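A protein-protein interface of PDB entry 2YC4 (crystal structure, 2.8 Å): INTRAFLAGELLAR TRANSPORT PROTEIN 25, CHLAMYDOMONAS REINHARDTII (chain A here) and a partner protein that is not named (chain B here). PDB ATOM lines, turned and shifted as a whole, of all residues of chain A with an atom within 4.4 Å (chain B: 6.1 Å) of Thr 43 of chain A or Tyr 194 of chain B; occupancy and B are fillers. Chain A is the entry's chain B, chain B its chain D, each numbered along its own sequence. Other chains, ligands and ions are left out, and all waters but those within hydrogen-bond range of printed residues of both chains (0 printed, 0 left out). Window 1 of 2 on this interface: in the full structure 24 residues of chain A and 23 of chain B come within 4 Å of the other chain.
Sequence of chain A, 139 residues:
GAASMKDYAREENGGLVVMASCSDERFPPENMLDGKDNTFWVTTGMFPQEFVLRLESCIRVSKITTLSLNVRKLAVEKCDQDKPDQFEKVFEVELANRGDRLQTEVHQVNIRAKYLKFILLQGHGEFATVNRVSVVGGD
OE2 of Glu 195 of chain B lies within salt-bridge range of NH2 of Arg 26 of chain A, 2.5 Å away. The side-chain hydroxyl of Tyr 194 of chain B is in hydrogen-bond range of the side-chain carboxylate of Asp 24 of chain A.
The backbone NH of Thr 43 of chain A lies within hydrogen-bond range of the backbone carbonyl oxygen of Ala 128 of chain A (2.9 Å). OD2 of Asp 24 of chain A is in salt-bridge range of NH2 of Arg 26 of chain A (2.9 Å). The side-chain sulfur (SG) of Cys 22 of chain A lies within hydrogen-bond range of the backbone NH (N) of Thr 44 of chain A (3.6 Å). The side-chain amide nitrogen (ND2) of Asn 193 of chain B lies close to the side-chain amino group (NZ) of Lys 197 of chain B (3.5 Å). OD1 of Asn 193 of chain B sits close to O of Phe 190 of chain B, at 3.0 Å.
CG of Asp 24 of chain A touches CB of Ala 17 of chain B (3.6 Å). Tyr 194 of chain B touches Arg 26 of chain A. OH of Tyr 194 of chain B touches CG1 of Val 42 of chain A, at 3.5 Å. O of Thr 43 of chain A touches CE1 of Tyr 194 of chain B, 3.7 Å away. Thr 44 of chain A touches Leu 19 of chain B (O to CB, 3.0 Å). Thr 44 of chain A touches Phe 190 of chain B. Tyr 194 of chain B touches Thr 44 of chain A (CE1 to CA, 3.9 Å). Phe 190 of chain B touches Phe 127 of chain A. CE1 of Phe 127 of chain A touches CD1 of Tyr 194 of chain B, 3.5 Å away. CG of Lys 197 of chain B touches CD2 of Phe 127 of chain A, at 3.8 Å.
Of the printed residues of chain B, Thr 44 of chain A touches Leu 19 (3.0 Å), Phe 190 (3.9 Å) and Tyr 194 (3.9 Å). Leu 120 of chain A touches none of the printed residues of chain B. Printed residues of chain A within 4 Å of Leu 19 of chain B: Thr 44. Arg 192 of chain B touches none of the printed residues of chain A. The nearest printed residue of chain A that does not touch Tyr 194 of chain B is Gly 45 of chain A (5.3 Å).
Of the 13 printed residues of chain B, 6 touch a printed residue of chain A. Hydrophobic or aromatic side chains of chain B within 4 Å of the printed part of chain A: Ala 17, Leu 19, Phe 190 and Tyr 194. Along chain A the printed residues that touch a printed residue of chain B span positions 24 to 127. Among the printed residues, Asp or Glu carboxylates within 4 Å of a Lys or Arg side-chain nitrogen of the other chain: Arg 26 of chain A with Glu 195 of chain B (2.5 Å).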
ATOM      1  N   CYS A  22     -26.740  30.787  -3.619  1.00  0.00           N
ATOM      2  CA  CYS A  22     -26.543  29.541  -2.906  1.00  0.00           C
ATOM      3  C   CYS A  22     -26.108  29.886  -1.500  1.00  0.00           C
ATOM      4  O   CYS A  22     -25.458  30.900  -1.294  1.00  0.00           O
ATOM      5  CB  CYS A  22     -25.485  28.693  -3.610  1.00  0.00           C
ATOM      6  SG  CYS A  22     -23.797  29.360  -3.573  1.00  0.00           S
ATOM      7  N   ASP A  24     -25.296  28.250   2.817  1.00  0.00           N
ATOM      8  CA  ASP A  24     -25.247  27.337   3.939  1.00  0.00           C
ATOM      9  C   ASP A  24     -25.313  28.211   5.192  1.00  0.00           C
ATOM     10  O   ASP A  24     -24.462  29.093   5.391  1.00  0.00           O
ATOM     11  CB  ASP A  24     -23.928  26.578   3.895  1.00  0.00           C
ATOM     12  CG  ASP A  24     -23.773  25.602   5.027  1.00  0.00           C
ATOM     13  OD1 ASP A  24     -24.399  25.782   6.095  1.00  0.00           O
ATOM     14  OD2 ASP A  24     -22.995  24.647   4.853  1.00  0.00           O
ATOM     15  N   ARG A  26     -24.284  28.089   7.782  1.00  0.00           N
ATOM     16  CA  ARG A  26     -23.044  28.120   8.549  1.00  0.00           C
ATOM     17  C   ARG A  26     -22.081  29.162   8.051  1.00  0.00           C
ATOM     18  O   ARG A  26     -21.088  29.449   8.714  1.00  0.00           O
ATOM     19  CB  ARG A  26     -22.327  26.772   8.502  1.00  0.00           C
ATOM     20  CG  ARG A  26     -22.823  25.754   9.481  1.00  0.00           C
ATOM     21  CD  ARG A  26     -22.024  24.500   9.306  1.00  0.00           C
ATOM     22  NE  ARG A  26     -22.134  23.999   7.944  1.00  0.00           N
ATOM     23  CZ  ARG A  26     -21.578  22.864   7.524  1.00  0.00           C
ATOM     24  NH1 ARG A  26     -20.874  22.125   8.383  1.00  0.00           N
ATOM     25  NH2 ARG A  26     -21.727  22.470   6.255  1.00  0.00           N
ATOM     26  N   TRP A  41     -18.320  33.638   3.215  1.00  0.00           N
ATOM     27  CA  TRP A  41     -19.435  33.022   2.537  1.00  0.00           C
ATOM     28  C   TRP A  41     -18.830  31.995   1.590  1.00  0.00           C
ATOM     29  O   TRP A  41     -17.791  32.247   0.972  1.00  0.00           O
ATOM     30  CB  TRP A  41     -20.207  34.076   1.763  1.00  0.00           C
ATOM     31  CG  TRP A  41     -21.251  33.543   0.860  1.00  0.00           C
ATOM     32  CD1 TRP A  41     -22.457  33.031   1.219  1.00  0.00           C
ATOM     33  CD2 TRP A  41     -21.204  33.503  -0.571  1.00  0.00           C
ATOM     34  NE1 TRP A  41     -23.173  32.660   0.101  1.00  0.00           N
ATOM     35  CE2 TRP A  41     -22.426  32.939  -1.014  1.00  0.00           C
ATOM     36  CE3 TRP A  41     -20.248  33.876  -1.525  1.00  0.00           C
ATOM     37  CZ2 TRP A  41     -22.713  32.741  -2.365  1.00  0.00           C
ATOM     38  CZ3 TRP A  41     -20.538  33.674  -2.868  1.00  0.00           C
ATOM     39  CH2 TRP A  41     -21.764  33.116  -3.271  1.00  0.00           C
ATOM     40  N   VAL A  42     -19.464  30.830   1.491  1.00  0.00           N
ATOM     41  CA  VAL A  42     -18.940  29.771   0.650  1.00  0.00           C
ATOM     42  C   VAL A  42     -20.004  29.335  -0.324  1.00  0.00           C
ATOM     43  O   VAL A  42     -21.195  29.333   0.010  1.00  0.00           O
ATOM     44  CB  VAL A  42     -18.499  28.557   1.492  1.00  0.00           C
ATOM     45  CG1 VAL A  42     -19.712  27.827   2.073  1.00  0.00           C
ATOM     46  CG2 VAL A  42     -17.593  27.616   0.673  1.00  0.00           C
ATOM     47  N   THR A  43     -19.562  28.971  -1.528  1.00  0.00           N
ATOM     48  CA  THR A  43     -20.460  28.430  -2.546  1.00  0.00           C
ATOM     49  C   THR A  43     -20.711  26.959  -2.229  1.00  0.00           C
ATOM     50  O   THR A  43     -19.892  26.326  -1.548  1.00  0.00           O
ATOM     51  CB  THR A  43     -19.907  28.625  -3.983  1.00  0.00           C
ATOM     52  OG1 THR A  43     -18.817  27.740  -4.232  1.00  0.00           O
ATOM     53  CG2 THR A  43     -19.401  30.025  -4.164  1.00  0.00           C
ATOM     54  N   THR A  44     -21.830  26.420  -2.718  1.00  0.00           N
ATOM     55  CA  THR A  44     -22.285  25.094  -2.328  1.00  0.00           C
ATOM     56  C   THR A  44     -22.222  24.088  -3.462  1.00  0.00           C
ATOM     57  O   THR A  44     -22.846  23.027  -3.409  1.00  0.00           O
ATOM     58  CB  THR A  44     -23.744  25.130  -1.834  1.00  0.00           C
ATOM     59  OG1 THR A  44     -24.587  25.672  -2.861  1.00  0.00           O
ATOM     60  CG2 THR A  44     -23.873  25.944  -0.548  1.00  0.00           C
ATOM     61  N   GLY A  45     -21.476  24.409  -4.502  1.00  0.00           N
ATOM     62  CA  GLY A  45     -21.492  23.569  -5.681  1.00  0.00           C
ATOM     63  C   GLY A  45     -21.038  24.331  -6.909  1.00  0.00           C
ATOM     64  O   GLY A  45     -20.010  25.020  -6.890  1.00  0.00           O
ATOM     65  N   PHE A  47     -20.728  26.349 -10.816  1.00  0.00           N
ATOM     66  CA  PHE A  47     -20.562  27.758 -11.206  1.00  0.00           C
ATOM     67  C   PHE A  47     -21.404  28.086 -12.459  1.00  0.00           C
ATOM     68  O   PHE A  47     -21.753  27.183 -13.232  1.00  0.00           O
ATOM     69  CB  PHE A  47     -19.093  28.124 -11.414  1.00  0.00           C
ATOM     70  CG  PHE A  47     -18.285  28.130 -10.154  1.00  0.00           C
ATOM     71  CD1 PHE A  47     -17.834  26.951  -9.597  1.00  0.00           C
ATOM     72  CD2 PHE A  47     -17.953  29.313  -9.536  1.00  0.00           C
ATOM     73  CE1 PHE A  47     -17.085  26.945  -8.445  1.00  0.00           C
ATOM     74  CE2 PHE A  47     -17.190  29.319  -8.356  1.00  0.00           C
ATOM     75  CZ  PHE A  47     -16.763  28.140  -7.820  1.00  0.00           C
ATOM     76  N   GLN A  49     -21.818  31.522  -9.667  1.00  0.00           N
ATOM     77  CA  GLN A  49     -22.632  31.859  -8.489  1.00  0.00           C
ATOM     78  C   GLN A  49     -22.603  33.365  -8.315  1.00  0.00           C
ATOM     79  O   GLN A  49     -21.624  34.018  -8.660  1.00  0.00           O
ATOM     80  CB  GLN A  49     -22.091  31.197  -7.225  1.00  0.00           C
ATOM     81  CG  GLN A  49     -21.958  29.669  -7.280  1.00  0.00           C
ATOM     82  CD  GLN A  49     -23.288  28.907  -7.234  1.00  0.00           C
ATOM     83  OE1 GLN A  49     -24.359  29.473  -6.963  1.00  0.00           O
ATOM     84  NE2 GLN A  49     -23.217  27.610  -7.511  1.00  0.00           N
ATOM     85  N   LEU A 120     -19.189  35.071  -9.309  1.00  0.00           N
ATOM     86  CA  LEU A 120     -18.089  34.129  -9.438  1.00  0.00           C
ATOM     87  C   LEU A 120     -18.383  33.267 -10.659  1.00  0.00           C
ATOM     88  O   LEU A 120     -19.208  32.321 -10.610  1.00  0.00           O
ATOM     89  CB  LEU A 120     -17.988  33.242  -8.199  1.00  0.00           C
ATOM     90  CG  LEU A 120     -17.579  33.870  -6.858  1.00  0.00           C
ATOM     91  CD1 LEU A 120     -18.325  35.156  -6.520  1.00  0.00           C
ATOM     92  CD2 LEU A 120     -17.769  32.855  -5.756  1.00  0.00           C
ATOM     93  N   PHE A 127     -15.527  24.445  -5.057  1.00  0.00           N
ATOM     94  CA  PHE A 127     -16.169  25.456  -4.234  1.00  0.00           C
ATOM     95  C   PHE A 127     -15.259  26.670  -4.086  1.00  0.00           C
ATOM     96  O   PHE A 127     -14.085  26.612  -4.435  1.00  0.00           O
ATOM     97  CB  PHE A 127     -16.501  24.872  -2.858  1.00  0.00           C
ATOM     98  CG  PHE A 127     -17.198  23.549  -2.912  1.00  0.00           C
ATOM     99  CD1 PHE A 127     -18.522  23.469  -3.281  1.00  0.00           C
ATOM    100  CD2 PHE A 127     -16.538  22.382  -2.563  1.00  0.00           C
ATOM    101  CE1 PHE A 127     -19.197  22.216  -3.325  1.00  0.00           C
ATOM    102  CE2 PHE A 127     -17.186  21.134  -2.604  1.00  0.00           C
ATOM    103  CZ  PHE A 127     -18.527  21.049  -2.994  1.00  0.00           C
ATOM    104  N   ALA A 128     -15.806  27.769  -3.567  1.00  0.00           N
ATOM    105  CA  ALA A 128     -15.030  28.989  -3.303  1.00  0.00           C
ATOM    106  C   ALA A 128     -15.610  29.799  -2.146  1.00  0.00           C
ATOM    107  O   ALA A 128     -16.737  29.536  -1.671  1.00  0.00           O
ATOM    108  CB  ALA A 128     -14.963  29.829  -4.532  1.00  0.00           C
ATOM    109  N   ALA B  17     -28.868  24.244   4.206  1.00  0.00           N
ATOM    110  CA  ALA B  17     -27.910  24.376   3.124  1.00  0.00           C
ATOM    111  C   ALA B  17     -28.410  23.561   1.946  1.00  0.00           C
ATOM    112  O   ALA B  17     -28.811  22.429   2.107  1.00  0.00           O
ATOM    113  CB  ALA B  17     -26.539  23.905   3.566  1.00  0.00           C
ATOM    114  N   LEU B  19     -26.808  22.287  -1.610  1.00  0.00           N
ATOM    115  CA  LEU B  19     -25.643  22.140  -2.470  1.00  0.00           C
ATOM    116  C   LEU B  19     -26.091  21.626  -3.829  1.00  0.00           C
ATOM    117  O   LEU B  19     -27.116  20.958  -3.944  1.00  0.00           O
ATOM    118  CB  LEU B  19     -24.649  21.137  -1.878  1.00  0.00           C
ATOM    119  CG  LEU B  19     -24.497  21.020  -0.358  1.00  0.00           C
ATOM    120  CD1 LEU B  19     -23.413  19.993  -0.033  1.00  0.00           C
ATOM    121  CD2 LEU B  19     -24.208  22.362   0.326  1.00  0.00           C
ATOM    122  N   THR B 189     -21.449  10.968  -1.537  1.00  0.00           N
ATOM    123  CA  THR B 189     -20.050  11.110  -1.860  1.00  0.00           C
ATOM    124  C   THR B 189     -19.688  12.579  -2.087  1.00  0.00           C
ATOM    125  O   THR B 189     -18.604  13.031  -1.723  1.00  0.00           O
ATOM    126  CB  THR B 189     -19.703  10.343  -3.121  1.00  0.00           C
ATOM    127  OG1 THR B 189     -20.216   9.008  -3.031  1.00  0.00           O
ATOM    128  CG2 THR B 189     -18.203  10.305  -3.301  1.00  0.00           C
ATOM    129  N   PHE B 190     -20.607  13.310  -2.706  1.00  0.00           N
ATOM    130  CA  PHE B 190     -20.453  14.734  -2.968  1.00  0.00           C
ATOM    131  C   PHE B 190     -20.566  15.559  -1.688  1.00  0.00           C
ATOM    132  O   PHE B 190     -19.772  16.482  -1.434  1.00  0.00           O
ATOM    133  CB  PHE B 190     -21.553  15.187  -3.917  1.00  0.00           C
ATOM    134  CG  PHE B 190     -21.620  16.667  -4.083  1.00  0.00           C
ATOM    135  CD1 PHE B 190     -20.511  17.373  -4.514  1.00  0.00           C
ATOM    136  CD2 PHE B 190     -22.787  17.357  -3.801  1.00  0.00           C
ATOM    137  CE1 PHE B 190     -20.571  18.742  -4.672  1.00  0.00           C
ATOM    138  CE2 PHE B 190     -22.850  18.725  -3.949  1.00  0.00           C
ATOM    139  CZ  PHE B 190     -21.742  19.417  -4.392  1.00  0.00           C
ATOM    140  N   TYR B 191     -21.591  15.241  -0.900  1.00  0.00           N
ATOM    141  CA  TYR B 191     -21.793  15.904   0.368  1.00  0.00           C
ATOM    142  C   TYR B 191     -20.484  15.916   1.110  1.00  0.00           C
ATOM    143  O   TYR B 191     -19.996  16.962   1.521  1.00  0.00           O
ATOM    144  CB  TYR B 191     -22.827  15.148   1.193  1.00  0.00           C
ATOM    145  CG  TYR B 191     -22.972  15.664   2.616  1.00  0.00           C
ATOM    146  CD1 TYR B 191     -23.384  16.963   2.860  1.00  0.00           C
ATOM    147  CD2 TYR B 191     -22.701  14.849   3.708  1.00  0.00           C
ATOM    148  CE1 TYR B 191     -23.520  17.446   4.148  1.00  0.00           C
ATOM    149  CE2 TYR B 191     -22.834  15.319   4.996  1.00  0.00           C
ATOM    150  CZ  TYR B 191     -23.249  16.627   5.218  1.00  0.00           C
ATOM    151  OH  TYR B 191     -23.411  17.133   6.502  1.00  0.00           O
ATOM    152  N   ARG B 192     -19.909  14.733   1.253  1.00  0.00           N
ATOM    153  CA  ARG B 192     -18.776  14.540   2.129  1.00  0.00           C
ATOM    154  C   ARG B 192     -17.565  15.370   1.795  1.00  0.00           C
ATOM    155  O   ARG B 192     -16.948  15.956   2.678  1.00  0.00           O
ATOM    156  CB  ARG B 192     -18.420  13.063   2.203  1.00  0.00           C
ATOM    157  CG  ARG B 192     -19.276  12.338   3.228  1.00  0.00           C
ATOM    158  CD  ARG B 192     -19.201  10.832   3.108  1.00  0.00           C
ATOM    159  NE  ARG B 192     -20.368  10.225   3.745  1.00  0.00           N
ATOM    160  CZ  ARG B 192     -20.505   8.926   4.003  1.00  0.00           C
ATOM    161  NH1 ARG B 192     -19.536   8.076   3.684  1.00  0.00           N
ATOM    162  NH2 ARG B 192     -21.613   8.483   4.588  1.00  0.00           N
ATOM    163  N   ASN B 193     -17.213  15.446   0.528  1.00  0.00           N
ATOM    164  CA  ASN B 193     -16.056  16.256   0.205  1.00  0.00           C
ATOM    165  C   ASN B 193     -16.373  17.761   0.164  1.00  0.00           C
ATOM    166  O   ASN B 193     -15.485  18.586   0.035  1.00  0.00           O
ATOM    167  CB  ASN B 193     -15.389  15.774  -1.077  1.00  0.00           C
ATOM    168  CG  ASN B 193     -15.998  16.380  -2.292  1.00  0.00           C
ATOM    169  OD1 ASN B 193     -17.069  15.955  -2.739  1.00  0.00           O
ATOM    170  ND2 ASN B 193     -15.329  17.395  -2.842  1.00  0.00           N
ATOM    171  N   TYR B 194     -17.647  18.103   0.289  1.00  0.00           N
ATOM    172  CA  TYR B 194     -18.027  19.480   0.511  1.00  0.00           C
ATOM    173  C   TYR B 194     -17.551  19.842   1.896  1.00  0.00           C
ATOM    174  O   TYR B 194     -16.734  20.741   2.084  1.00  0.00           O
ATOM    175  CB  TYR B 194     -19.544  19.639   0.428  1.00  0.00           C
ATOM    176  CG  TYR B 194     -20.030  20.990   0.912  1.00  0.00           C
ATOM    177  CD1 TYR B 194     -19.902  22.119   0.120  1.00  0.00           C
ATOM    178  CD2 TYR B 194     -20.607  21.140   2.164  1.00  0.00           C
ATOM    179  CE1 TYR B 194     -20.329  23.369   0.563  1.00  0.00           C
ATOM    180  CE2 TYR B 194     -21.045  22.383   2.613  1.00  0.00           C
ATOM    181  CZ  TYR B 194     -20.900  23.495   1.809  1.00  0.00           C
ATOM    182  OH  TYR B 194     -21.326  24.733   2.243  1.00  0.00           O
ATOM    183  N   GLU B 195     -18.060  19.093   2.865  1.00  0.00           N
ATOM    184  CA  GLU B 195     -17.672  19.213   4.263  1.00  0.00           C
ATOM    185  C   GLU B 195     -16.140  19.246   4.493  1.00  0.00           C
ATOM    186  O   GLU B 195     -15.635  19.970   5.378  1.00  0.00           O
ATOM    187  CB  GLU B 195     -18.313  18.064   5.024  1.00  0.00           C
ATOM    188  CG  GLU B 195     -19.793  18.203   5.155  1.00  0.00           C
ATOM    189  CD  GLU B 195     -20.144  19.330   6.088  1.00  0.00           C
ATOM    190  OE1 GLU B 195     -19.379  19.524   7.051  1.00  0.00           O
ATOM    191  OE2 GLU B 195     -21.159  20.027   5.860  1.00  0.00           O
ATOM    192  N   ASP B 196     -15.436  18.436   3.701  1.00  0.00           N
ATOM    193  CA  ASP B 196     -13.992  18.378   3.652  1.00  0.00           C
ATOM    194  C   ASP B 196     -13.450  19.740   3.313  1.00  0.00           C
ATOM    195  O   ASP B 196     -12.686  20.338   4.068  1.00  0.00           O
ATOM    196  CB  ASP B 196     -13.589  17.483   2.489  1.00  0.00           C
ATOM    197  CG  ASP B 196     -13.314  16.067   2.902  1.00  0.00           C
ATOM    198  OD1 ASP B 196     -14.242  15.386   3.384  1.00  0.00           O
ATOM    199  OD2 ASP B 196     -12.160  15.632   2.718  1.00  0.00           O
ATOM    200  N   LYS B 197     -13.835  20.209   2.133  1.00  0.00           N
ATOM    201  CA  LYS B 197     -13.329  21.462   1.591  1.00  0.00           C
ATOM    202  C   LYS B 197     -13.668  22.633   2.500  1.00  0.00           C
ATOM    203  O   LYS B 197     -12.841  23.516   2.732  1.00  0.00           O
ATOM    204  CB  LYS B 197     -13.902  21.716   0.191  1.00  0.00           C
ATOM    205  CG  LYS B 197     -13.600  20.633  -0.826  1.00  0.00           C
ATOM    206  CD  LYS B 197     -12.114  20.435  -1.011  1.00  0.00           C
ATOM    207  CE  LYS B 197     -11.821  19.290  -1.969  1.00  0.00           C
ATOM    208  NZ  LYS B 197     -12.538  19.438  -3.297  1.00  0.00           N
ATOM    209  N   VAL B 198     -14.900  22.634   2.993  1.00  0.00           N
ATOM    210  CA  VAL B 198     -15.378  23.672   3.896  1.00  0.00           C
ATOM    211  C   VAL B 198     -14.557  23.772   5.185  1.00  0.00           C
ATOM    212  O   VAL B 198     -14.350  24.866   5.708  1.00  0.00           O
ATOM    213  CB  VAL B 198     -16.854  23.437   4.265  1.00  0.00           C
ATOM    214  CG1 VAL B 198     -17.332  24.475   5.240  1.00  0.00           C
ATOM    215  CG2 VAL B 198     -17.707  23.474   3.029  1.00  0.00           C
ATOM    216  N   ALA B 199     -14.110  22.635   5.708  1.00  0.00           N
ATOM    217  CA  ALA B 199     -13.313  22.638   6.917  1.00  0.00           C
ATOM    218  C   ALA B 199     -11.919  23.131   6.574  1.00  0.00           C
ATOM    219  O   ALA B 199     -11.337  23.963   7.275  1.00  0.00           O
ATOM    220  CB  ALA B 199     -13.267  21.261   7.493  1.00  0.00           C
